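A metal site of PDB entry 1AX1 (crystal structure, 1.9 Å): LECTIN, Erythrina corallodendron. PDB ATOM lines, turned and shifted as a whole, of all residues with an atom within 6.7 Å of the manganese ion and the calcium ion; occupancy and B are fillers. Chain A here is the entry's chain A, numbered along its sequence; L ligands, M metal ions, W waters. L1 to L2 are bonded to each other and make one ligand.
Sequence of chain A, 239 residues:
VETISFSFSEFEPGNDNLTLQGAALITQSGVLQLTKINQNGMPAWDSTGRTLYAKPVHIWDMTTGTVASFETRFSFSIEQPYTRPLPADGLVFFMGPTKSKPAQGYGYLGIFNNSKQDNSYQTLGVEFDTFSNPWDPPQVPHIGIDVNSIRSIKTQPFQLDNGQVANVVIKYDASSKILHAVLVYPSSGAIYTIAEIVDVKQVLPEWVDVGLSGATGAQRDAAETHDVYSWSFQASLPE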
ATOM      1  N   ASP A  89      -7.325  14.690 -30.656  1.00  0.00           N
ATOM      2  CA  ASP A  89      -6.302  13.668 -30.435  1.00  0.00           C
ATOM      3  C   ASP A  89      -6.857  12.255 -30.567  1.00  0.00           C
ATOM      4  O   ASP A  89      -6.112  11.293 -30.800  1.00  0.00           O
ATOM      5  CB  ASP A  89      -5.675  13.817 -29.047  1.00  0.00           C
ATOM      6  CG  ASP A  89      -4.442  14.689 -29.056  1.00  0.00           C
ATOM      7  OD1 ASP A  89      -3.373  14.202 -29.469  1.00  0.00           O
ATOM      8  OD2 ASP A  89      -4.558  15.868 -28.666  1.00  0.00           O
ATOM      9  N   TYR A 106      -5.043  15.696 -24.278  1.00  0.00           N
ATOM     10  CA  TYR A 106      -4.215  15.614 -25.477  1.00  0.00           C
ATOM     11  C   TYR A 106      -3.913  14.164 -25.859  1.00  0.00           C
ATOM     12  O   TYR A 106      -4.821  13.323 -25.860  1.00  0.00           O
ATOM     13  CB  TYR A 106      -2.909  16.410 -25.303  1.00  0.00           C
ATOM     14  CG  TYR A 106      -3.122  17.783 -24.723  1.00  0.00           C
ATOM     15  CD1 TYR A 106      -4.108  18.626 -25.226  1.00  0.00           C
ATOM     16  CD2 TYR A 106      -2.359  18.227 -23.648  1.00  0.00           C
ATOM     17  CE1 TYR A 106      -4.347  19.874 -24.654  1.00  0.00           C
ATOM     18  CE2 TYR A 106      -2.590  19.457 -23.067  1.00  0.00           C
ATOM     19  CZ  TYR A 106      -3.577  20.278 -23.571  1.00  0.00           C
ATOM     20  OH  TYR A 106      -3.777  21.511 -23.004  1.00  0.00           O
ATOM     21  N   GLY A 107      -2.652  13.888 -26.202  1.00  0.00           N
ATOM     22  CA  GLY A 107      -2.227  12.562 -26.599  1.00  0.00           C
ATOM     23  C   GLY A 107      -2.447  11.485 -25.561  1.00  0.00           C
ATOM     24  O   GLY A 107      -2.377  10.298 -25.872  1.00  0.00           O
ATOM     25  N   TYR A 108      -2.706  11.884 -24.312  1.00  0.00           N
ATOM     26  CA  TYR A 108      -2.945  10.937 -23.227  1.00  0.00           C
ATOM     27  C   TYR A 108      -4.403  10.518 -23.145  1.00  0.00           C
ATOM     28  O   TYR A 108      -4.765   9.648 -22.342  1.00  0.00           O
ATOM     29  CB  TYR A 108      -2.420  11.491 -21.911  1.00  0.00           C
ATOM     30  CG  TYR A 108      -0.928  11.737 -21.973  1.00  0.00           C
ATOM     31  CD1 TYR A 108      -0.049  10.688 -22.259  1.00  0.00           C
ATOM     32  CD2 TYR A 108      -0.401  13.017 -21.822  1.00  0.00           C
ATOM     33  CE1 TYR A 108       1.317  10.911 -22.390  1.00  0.00           C
ATOM     34  CE2 TYR A 108       0.965  13.240 -21.953  1.00  0.00           C
ATOM     35  CZ  TYR A 108       1.810  12.184 -22.242  1.00  0.00           C
ATOM     36  OH  TYR A 108       3.163  12.412 -22.372  1.00  0.00           O
ATOM     37  N   LEU A 109      -5.223  11.146 -23.989  1.00  0.00           N
ATOM     38  CA  LEU A 109      -6.640  10.847 -24.126  1.00  0.00           C
ATOM     39  C   LEU A 109      -7.522  10.908 -22.867  1.00  0.00           C
ATOM     40  O   LEU A 109      -8.642  10.406 -22.874  1.00  0.00           O
ATOM     41  CB  LEU A 109      -6.810   9.482 -24.826  1.00  0.00           C
ATOM     42  CG  LEU A 109      -6.050   9.290 -26.148  1.00  0.00           C
ATOM     43  CD1 LEU A 109      -6.140   7.847 -26.605  1.00  0.00           C
ATOM     44  CD2 LEU A 109      -6.592  10.236 -27.222  1.00  0.00           C
ATOM     45  N   GLU A 127      -8.057   2.378 -28.094  1.00  0.00           N
ATOM     46  CA  GLU A 127      -8.062   3.723 -28.644  1.00  0.00           C
ATOM     47  C   GLU A 127      -8.307   3.825 -30.142  1.00  0.00           C
ATOM     48  O   GLU A 127      -8.120   2.876 -30.900  1.00  0.00           O
ATOM     49  CB  GLU A 127      -6.747   4.412 -28.313  1.00  0.00           C
ATOM     50  CG  GLU A 127      -5.540   3.707 -28.932  1.00  0.00           C
ATOM     51  CD  GLU A 127      -4.243   4.469 -28.778  1.00  0.00           C
ATOM     52  OE1 GLU A 127      -3.938   4.907 -27.662  1.00  0.00           O
ATOM     53  OE2 GLU A 127      -3.533   4.626 -29.793  1.00  0.00           O
ATOM     54  N   ASP A 129      -6.993   6.601 -32.176  1.00  0.00           N
ATOM     55  CA  ASP A 129      -6.000   7.662 -32.185  1.00  0.00           C
ATOM     56  C   ASP A 129      -5.859   8.406 -33.509  1.00  0.00           C
ATOM     57  O   ASP A 129      -5.457   7.818 -34.511  1.00  0.00           O
ATOM     58  CB  ASP A 129      -4.666   7.035 -31.782  1.00  0.00           C
ATOM     59  CG  ASP A 129      -3.661   8.046 -31.291  1.00  0.00           C
ATOM     60  OD1 ASP A 129      -3.805   9.261 -31.535  1.00  0.00           O
ATOM     61  OD2 ASP A 129      -2.694   7.608 -30.640  1.00  0.00           O
ATOM     62  N   THR A 130      -6.091   9.708 -33.474  1.00  0.00           N
ATOM     63  CA  THR A 130      -6.024  10.533 -34.679  1.00  0.00           C
ATOM     64  C   THR A 130      -4.773  11.409 -34.844  1.00  0.00           C
ATOM     65  O   THR A 130      -4.608  12.041 -35.893  1.00  0.00           O
ATOM     66  CB  THR A 130      -7.265  11.434 -34.808  1.00  0.00           C
ATOM     67  OG1 THR A 130      -7.353  12.306 -33.673  1.00  0.00           O
ATOM     68  CG2 THR A 130      -8.538  10.589 -34.888  1.00  0.00           C
ATOM     69  N   PHE A 131      -3.919  11.465 -33.827  1.00  0.00           N
ATOM     70  CA  PHE A 131      -2.701  12.269 -33.914  1.00  0.00           C
ATOM     71  C   PHE A 131      -1.486  11.435 -33.557  1.00  0.00           C
ATOM     72  O   PHE A 131      -1.464  10.761 -32.530  1.00  0.00           O
ATOM     73  CB  PHE A 131      -2.786  13.495 -32.995  1.00  0.00           C
ATOM     74  CG  PHE A 131      -1.567  14.375 -33.069  1.00  0.00           C
ATOM     75  CD1 PHE A 131      -0.465  14.140 -32.254  1.00  0.00           C
ATOM     76  CD2 PHE A 131      -1.503  15.421 -33.991  1.00  0.00           C
ATOM     77  CE1 PHE A 131       0.681  14.916 -32.336  1.00  0.00           C
ATOM     78  CE2 PHE A 131      -0.366  16.216 -34.081  1.00  0.00           C
ATOM     79  CZ  PHE A 131       0.734  15.954 -33.253  1.00  0.00           C
ATOM     80  N   SER A 132      -0.463  11.525 -34.392  1.00  0.00           N
ATOM     81  CA  SER A 132       0.771  10.775 -34.192  1.00  0.00           C
ATOM     82  C   SER A 132       1.781  11.442 -33.239  1.00  0.00           C
ATOM     83  O   SER A 132       2.488  12.376 -33.626  1.00  0.00           O
ATOM     84  CB  SER A 132       1.411  10.465 -35.550  1.00  0.00           C
ATOM     85  OG  SER A 132       2.435   9.500 -35.422  1.00  0.00           O
ATOM     86  N   ASN A 133       1.795  10.978 -31.985  1.00  0.00           N
ATOM     87  CA  ASN A 133       2.717  11.474 -30.959  1.00  0.00           C
ATOM     88  C   ASN A 133       4.031  10.706 -31.126  1.00  0.00           C
ATOM     89  O   ASN A 133       4.110   9.768 -31.910  1.00  0.00           O
ATOM     90  CB  ASN A 133       2.137  11.223 -29.563  1.00  0.00           C
ATOM     91  CG  ASN A 133       0.843  11.979 -29.324  1.00  0.00           C
ATOM     92  OD1 ASN A 133      -0.244  11.453 -29.528  1.00  0.00           O
ATOM     93  ND2 ASN A 133       0.959  13.215 -28.868  1.00  0.00           N
ATOM     94  N   TRP A 135       5.377   8.524 -29.355  1.00  0.00           N
ATOM     95  CA  TRP A 135       5.232   7.123 -28.946  1.00  0.00           C
ATOM     96  C   TRP A 135       4.319   6.330 -29.892  1.00  0.00           C
ATOM     97  O   TRP A 135       4.129   5.126 -29.713  1.00  0.00           O
ATOM     98  CB  TRP A 135       4.680   7.045 -27.517  1.00  0.00           C
ATOM     99  CG  TRP A 135       3.370   7.768 -27.359  1.00  0.00           C
ATOM    100  CD1 TRP A 135       2.131   7.346 -27.788  1.00  0.00           C
ATOM    101  CD2 TRP A 135       3.162   9.040 -26.732  1.00  0.00           C
ATOM    102  NE1 TRP A 135       1.173   8.278 -27.461  1.00  0.00           N
ATOM    103  CE2 TRP A 135       1.785   9.329 -26.821  1.00  0.00           C
ATOM    104  CE3 TRP A 135       4.011   9.963 -26.123  1.00  0.00           C
ATOM    105  CZ2 TRP A 135       1.220  10.512 -26.304  1.00  0.00           C
ATOM    106  CZ3 TRP A 135       3.463  11.149 -25.604  1.00  0.00           C
ATOM    107  CH2 TRP A 135       2.087  11.407 -25.705  1.00  0.00           C
ATOM    108  N   ASP A 136       3.737   7.006 -30.876  1.00  0.00           N
ATOM    109  CA  ASP A 136       2.823   6.387 -31.826  1.00  0.00           C
ATOM    110  C   ASP A 136       3.460   5.956 -33.131  1.00  0.00           C
ATOM    111  O   ASP A 136       4.554   6.406 -33.489  1.00  0.00           O
ATOM    112  CB  ASP A 136       1.726   7.377 -32.217  1.00  0.00           C
ATOM    113  CG  ASP A 136       0.658   7.507 -31.174  1.00  0.00           C
ATOM    114  OD1 ASP A 136       0.283   6.469 -30.589  1.00  0.00           O
ATOM    115  OD2 ASP A 136       0.180   8.644 -30.951  1.00  0.00           O
ATOM    116  N   PRO A 137       2.806   5.020 -33.849  1.00  0.00           N
ATOM    117  CA  PRO A 137       3.344   4.603 -35.134  1.00  0.00           C
ATOM    118  C   PRO A 137       3.074   5.824 -36.031  1.00  0.00           C
ATOM    119  O   PRO A 137       2.262   6.689 -35.669  1.00  0.00           O
ATOM    120  CB  PRO A 137       2.458   3.403 -35.506  1.00  0.00           C
ATOM    121  CG  PRO A 137       1.209   3.613 -34.713  1.00  0.00           C
ATOM    122  CD  PRO A 137       1.741   4.109 -33.403  1.00  0.00           C
ATOM    123  N   VAL A 140      -1.843   7.401 -38.926  1.00  0.00           N
ATOM    124  CA  VAL A 140      -3.005   7.840 -38.170  1.00  0.00           C
ATOM    125  C   VAL A 140      -4.117   8.063 -39.193  1.00  0.00           C
ATOM    126  O   VAL A 140      -3.847   8.449 -40.330  1.00  0.00           O
ATOM    127  CB  VAL A 140      -2.771   9.136 -37.360  1.00  0.00           C
ATOM    128  CG1 VAL A 140      -1.953   8.848 -36.115  1.00  0.00           C
ATOM    129  CG2 VAL A 140      -2.092  10.188 -38.224  1.00  0.00           C
ATOM    130  N   HIS A 142      -5.382   5.275 -36.110  1.00  0.00           N
ATOM    131  CA  HIS A 142      -5.118   3.868 -35.837  1.00  0.00           C
ATOM    132  C   HIS A 142      -5.861   3.411 -34.592  1.00  0.00           C
ATOM    133  O   HIS A 142      -6.174   4.207 -33.703  1.00  0.00           O
ATOM    134  CB  HIS A 142      -3.617   3.567 -35.707  1.00  0.00           C
ATOM    135  CG  HIS A 142      -2.931   4.306 -34.586  1.00  0.00           C
ATOM    136  ND1 HIS A 142      -2.196   5.452 -34.768  1.00  0.00           N
ATOM    137  CD2 HIS A 142      -2.874   4.039 -33.260  1.00  0.00           C
ATOM    138  CE1 HIS A 142      -1.721   5.843 -33.571  1.00  0.00           C
ATOM    139  NE2 HIS A 142      -2.110   5.015 -32.632  1.00  0.00           N
ATOM    140  N   ILE A 143      -6.209   2.127 -34.601  1.00  0.00           N
ATOM    141  CA  ILE A 143      -6.864   1.506 -33.460  1.00  0.00           C
ATOM    142  C   ILE A 143      -5.673   1.006 -32.628  1.00  0.00           C
ATOM    143  O   ILE A 143      -4.649   0.592 -33.188  1.00  0.00           O
ATOM    144  CB  ILE A 143      -7.712   0.283 -33.878  1.00  0.00           C
ATOM    145  CG1 ILE A 143      -8.728   0.690 -34.953  1.00  0.00           C
ATOM    146  CG2 ILE A 143      -8.446  -0.295 -32.661  1.00  0.00           C
ATOM    147  CD1 ILE A 143      -9.401  -0.478 -35.643  1.00  0.00           C
ATOM    148  N   GLY A 144      -5.786   1.072 -31.311  1.00  0.00           N
ATOM    149  CA  GLY A 144      -4.707   0.601 -30.484  1.00  0.00           C
ATOM    150  C   GLY A 144      -5.198  -0.059 -29.214  1.00  0.00           C
ATOM    151  O   GLY A 144      -6.226   0.329 -28.672  1.00  0.00           O
ATOM    152  N   ASP A 146      -4.301  -0.582 -25.526  1.00  0.00           N
ATOM    153  CA  ASP A 146      -3.464  -0.002 -24.469  1.00  0.00           C
ATOM    154  C   ASP A 146      -3.561  -0.783 -23.158  1.00  0.00           C
ATOM    155  O   ASP A 146      -4.658  -0.974 -22.623  1.00  0.00           O
ATOM    156  CB  ASP A 146      -3.875   1.448 -24.208  1.00  0.00           C
ATOM    157  CG  ASP A 146      -3.792   2.322 -25.440  1.00  0.00           C
ATOM    158  OD1 ASP A 146      -3.227   1.901 -26.463  1.00  0.00           O
ATOM    159  OD2 ASP A 146      -4.280   3.460 -25.398  1.00  0.00           O
ATOM    160  N   ILE A 150       0.007   4.408 -22.800  1.00  0.00           N
ATOM    161  CA  ILE A 150      -0.525   5.038 -24.003  1.00  0.00           C
ATOM    162  C   ILE A 150       0.219   4.460 -25.226  1.00  0.00           C
ATOM    163  O   ILE A 150      -0.222   4.599 -26.365  1.00  0.00           O
ATOM    164  CB  ILE A 150      -0.404   6.598 -23.933  1.00  0.00           C
ATOM    165  CG1 ILE A 150      -1.237   7.246 -25.041  1.00  0.00           C
ATOM    166  CG2 ILE A 150       1.052   7.033 -23.965  1.00  0.00           C
ATOM    167  CD1 ILE A 150      -2.745   7.044 -24.888  1.00  0.00           C
ATOM    168  N   ARG A 151       1.341   3.795 -24.966  1.00  0.00           N
ATOM    169  CA  ARG A 151       2.127   3.147 -26.017  1.00  0.00           C
ATOM    170  C   ARG A 151       1.488   1.776 -26.224  1.00  0.00           C
ATOM    171  O   ARG A 151       1.793   0.827 -25.514  1.00  0.00           O
ATOM    172  CB  ARG A 151       3.576   2.947 -25.564  1.00  0.00           C
ATOM    173  CG  ARG A 151       4.312   4.209 -25.178  1.00  0.00           C
ATOM    174  CD  ARG A 151       5.798   3.925 -25.049  1.00  0.00           C
ATOM    175  NE  ARG A 151       6.279   4.015 -23.668  1.00  0.00           N
ATOM    176  CZ  ARG A 151       6.717   2.991 -22.947  1.00  0.00           C
ATOM    177  NH1 ARG A 151       6.729   1.762 -23.453  1.00  0.00           N
ATOM    178  NH2 ARG A 151       7.132   3.195 -21.705  1.00  0.00           N
ATOM    179  N   SER A 152       0.612   1.681 -27.233  1.00  0.00           N
ATOM    180  CA  SER A 152      -0.115   0.447 -27.518  1.00  0.00           C
ATOM    181  C   SER A 152       0.752  -0.788 -27.692  1.00  0.00           C
ATOM    182  O   SER A 152       1.868  -0.698 -28.196  1.00  0.00           O
ATOM    183  CB  SER A 152      -0.950   0.625 -28.789  1.00  0.00           C
ATOM    184  OG  SER A 152      -1.698   1.812 -28.722  1.00  0.00           O
ATOM    185  N   THR A 155      -1.179  -2.229 -32.737  1.00  0.00           N
ATOM    186  CA  THR A 155      -1.787  -1.123 -33.474  1.00  0.00           C
ATOM    187  C   THR A 155      -2.333  -1.559 -34.838  1.00  0.00           C
ATOM    188  O   THR A 155      -1.817  -2.499 -35.455  1.00  0.00           O
ATOM    189  CB  THR A 155      -0.753   0.046 -33.609  1.00  0.00           C
ATOM    190  OG1 THR A 155      -1.033   1.049 -32.630  1.00  0.00           O
ATOM    191  CG2 THR A 155      -0.745   0.646 -34.979  1.00  0.00           C
HETATM  192  C1  LIG L   1       2.519  22.694 -29.392  1.00  0.00           C
HETATM  193  C2  LIG L   1       1.542  21.588 -29.024  1.00  0.00           C
HETATM  194  C3  LIG L   1       2.292  20.284 -28.741  1.00  0.00           C
HETATM  195  C4  LIG L   1       3.388  20.537 -27.704  1.00  0.00           C
HETATM  196  C5  LIG L   1       4.243  19.321 -27.412  1.00  0.00           C
HETATM  197  C6  LIG L   1       3.584  22.818 -28.312  1.00  0.00           C
HETATM  198  O1  LIG L   1       4.525  23.761 -28.695  1.00  0.00           O
HETATM  199  O2  LIG L   1       1.820  23.924 -29.536  1.00  0.00           O
HETATM  200  O3  LIG L   1       0.624  21.407 -30.094  1.00  0.00           O
HETATM  201  O4  LIG L   1       1.385  19.294 -28.209  1.00  0.00           O
HETATM  202  O5  LIG L   1       4.272  21.574 -28.151  1.00  0.00           O
HETATM  203  O6  LIG L   1       4.514  18.584 -28.603  1.00  0.00           O
HETATM  204  C1  LG2 L   2       0.842  18.371 -29.096  1.00  0.00           C
HETATM  205  C2  LG2 L   2       0.247  17.218 -28.276  1.00  0.00           C
HETATM  206  C3  LG2 L   2      -0.528  16.259 -29.191  1.00  0.00           C
HETATM  207  C4  LG2 L   2      -1.591  17.059 -29.959  1.00  0.00           C
HETATM  208  C5  LG2 L   2      -0.875  18.155 -30.739  1.00  0.00           C
HETATM  209  C6  LG2 L   2      -1.825  19.005 -31.556  1.00  0.00           C
HETATM  210  O1  LG2 L   2       1.281  16.511 -27.602  1.00  0.00           O
HETATM  211  O2  LG2 L   2      -1.155  15.252 -28.416  1.00  0.00           O
HETATM  212  O3  LG2 L   2      -2.520  17.629 -29.056  1.00  0.00           O
HETATM  213  O4  LG2 L   2      -0.190  19.044 -29.834  1.00  0.00           O
HETATM  214  O5  LG2 L   2      -1.113  20.005 -32.258  1.00  0.00           O
HETATM  215 MN    MN M   1      -1.743   5.664 -30.461  1.00  0.00          MN
HETATM  216 CA    CA M   2      -1.773   9.889 -30.395  1.00  0.00          CA
HETATM  217  O   HOH W   1      -1.507   6.132 -28.109  1.00  0.00           O
HETATM  218  O   HOH W   2      -1.779   9.026 -28.211  1.00  0.00           O
HETATM  219  O   HOH W   3      -3.241  11.518 -29.931  1.00  0.00           O
HETATM  220  O   HOH W   4      -0.681   3.794 -30.240  1.00  0.00           O
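An oxygen (O2) of LG2 L2 is in hydrogen-bond range of the side-chain amide nitrogen (ND2) of Asn 133, 3.0 Å away.
N of Gly 107 sits at hydrogen-bond distance from O2 of LG2 L2 (3.0 Å).
OD1 of Asp 89 is in hydrogen-bond range of O2 of LG2 L2 (2.7 Å).
The side-chain carboxylate (OE1) of Glu 127 lies close to the side-chain carboxylate (OD2) of Asp 146 (2.7 Å).
O of Gly 144 is in hydrogen-bond range of N of Glu 127, 2.8 Å away.
Four residues have an atom within 4 Å of the manganese ion: Glu 127, Asp 129, Asp 136 and His 142.
The nearest printed residue that does not touch the manganese ion is Ser 152 (4.2 Å).
Four residues have an atom within 4 Å of the calcium ion: Asp 129, Phe 131, Asn 133 and Asp 136.
Water W4 is bound to the manganese ion, 2.2 Å away.
OD2 of Asp 129 is bound to the manganese ion, 2.2 Å away.
The manganese ion is bound by OE2 of Glu 127 (2.2 Å).
The side-chain carboxylate (OD1) of Asp 136 binds the manganese ion (2.2 Å).
NE2 of His 142 is bound to the manganese ion (2.3 Å).
Water W1 is bound to the manganese ion (2.4 Å).
The calcium ion is bound by water W3 (2.2 Å), O of Phe 131 (2.3 Å), water W2 (2.3 Å), OD1 of Asn 133 (2.4 Å), OD2 of Asp 136 (2.4 Å), OD1 of Asp 129 (2.4 Å) and OD2 of Asp 129 (2.5 Å).
The calcium ion has seven donor atoms within binding distance.
Water W1 lies within hydrogen-bond range of O of Ile 150, OE1 of Glu 127 and NE1 of Trp 135.
Water W2 bridges O of Gly 107 (2.7 Å) and NE1 of Trp 135 (3.1 Å).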
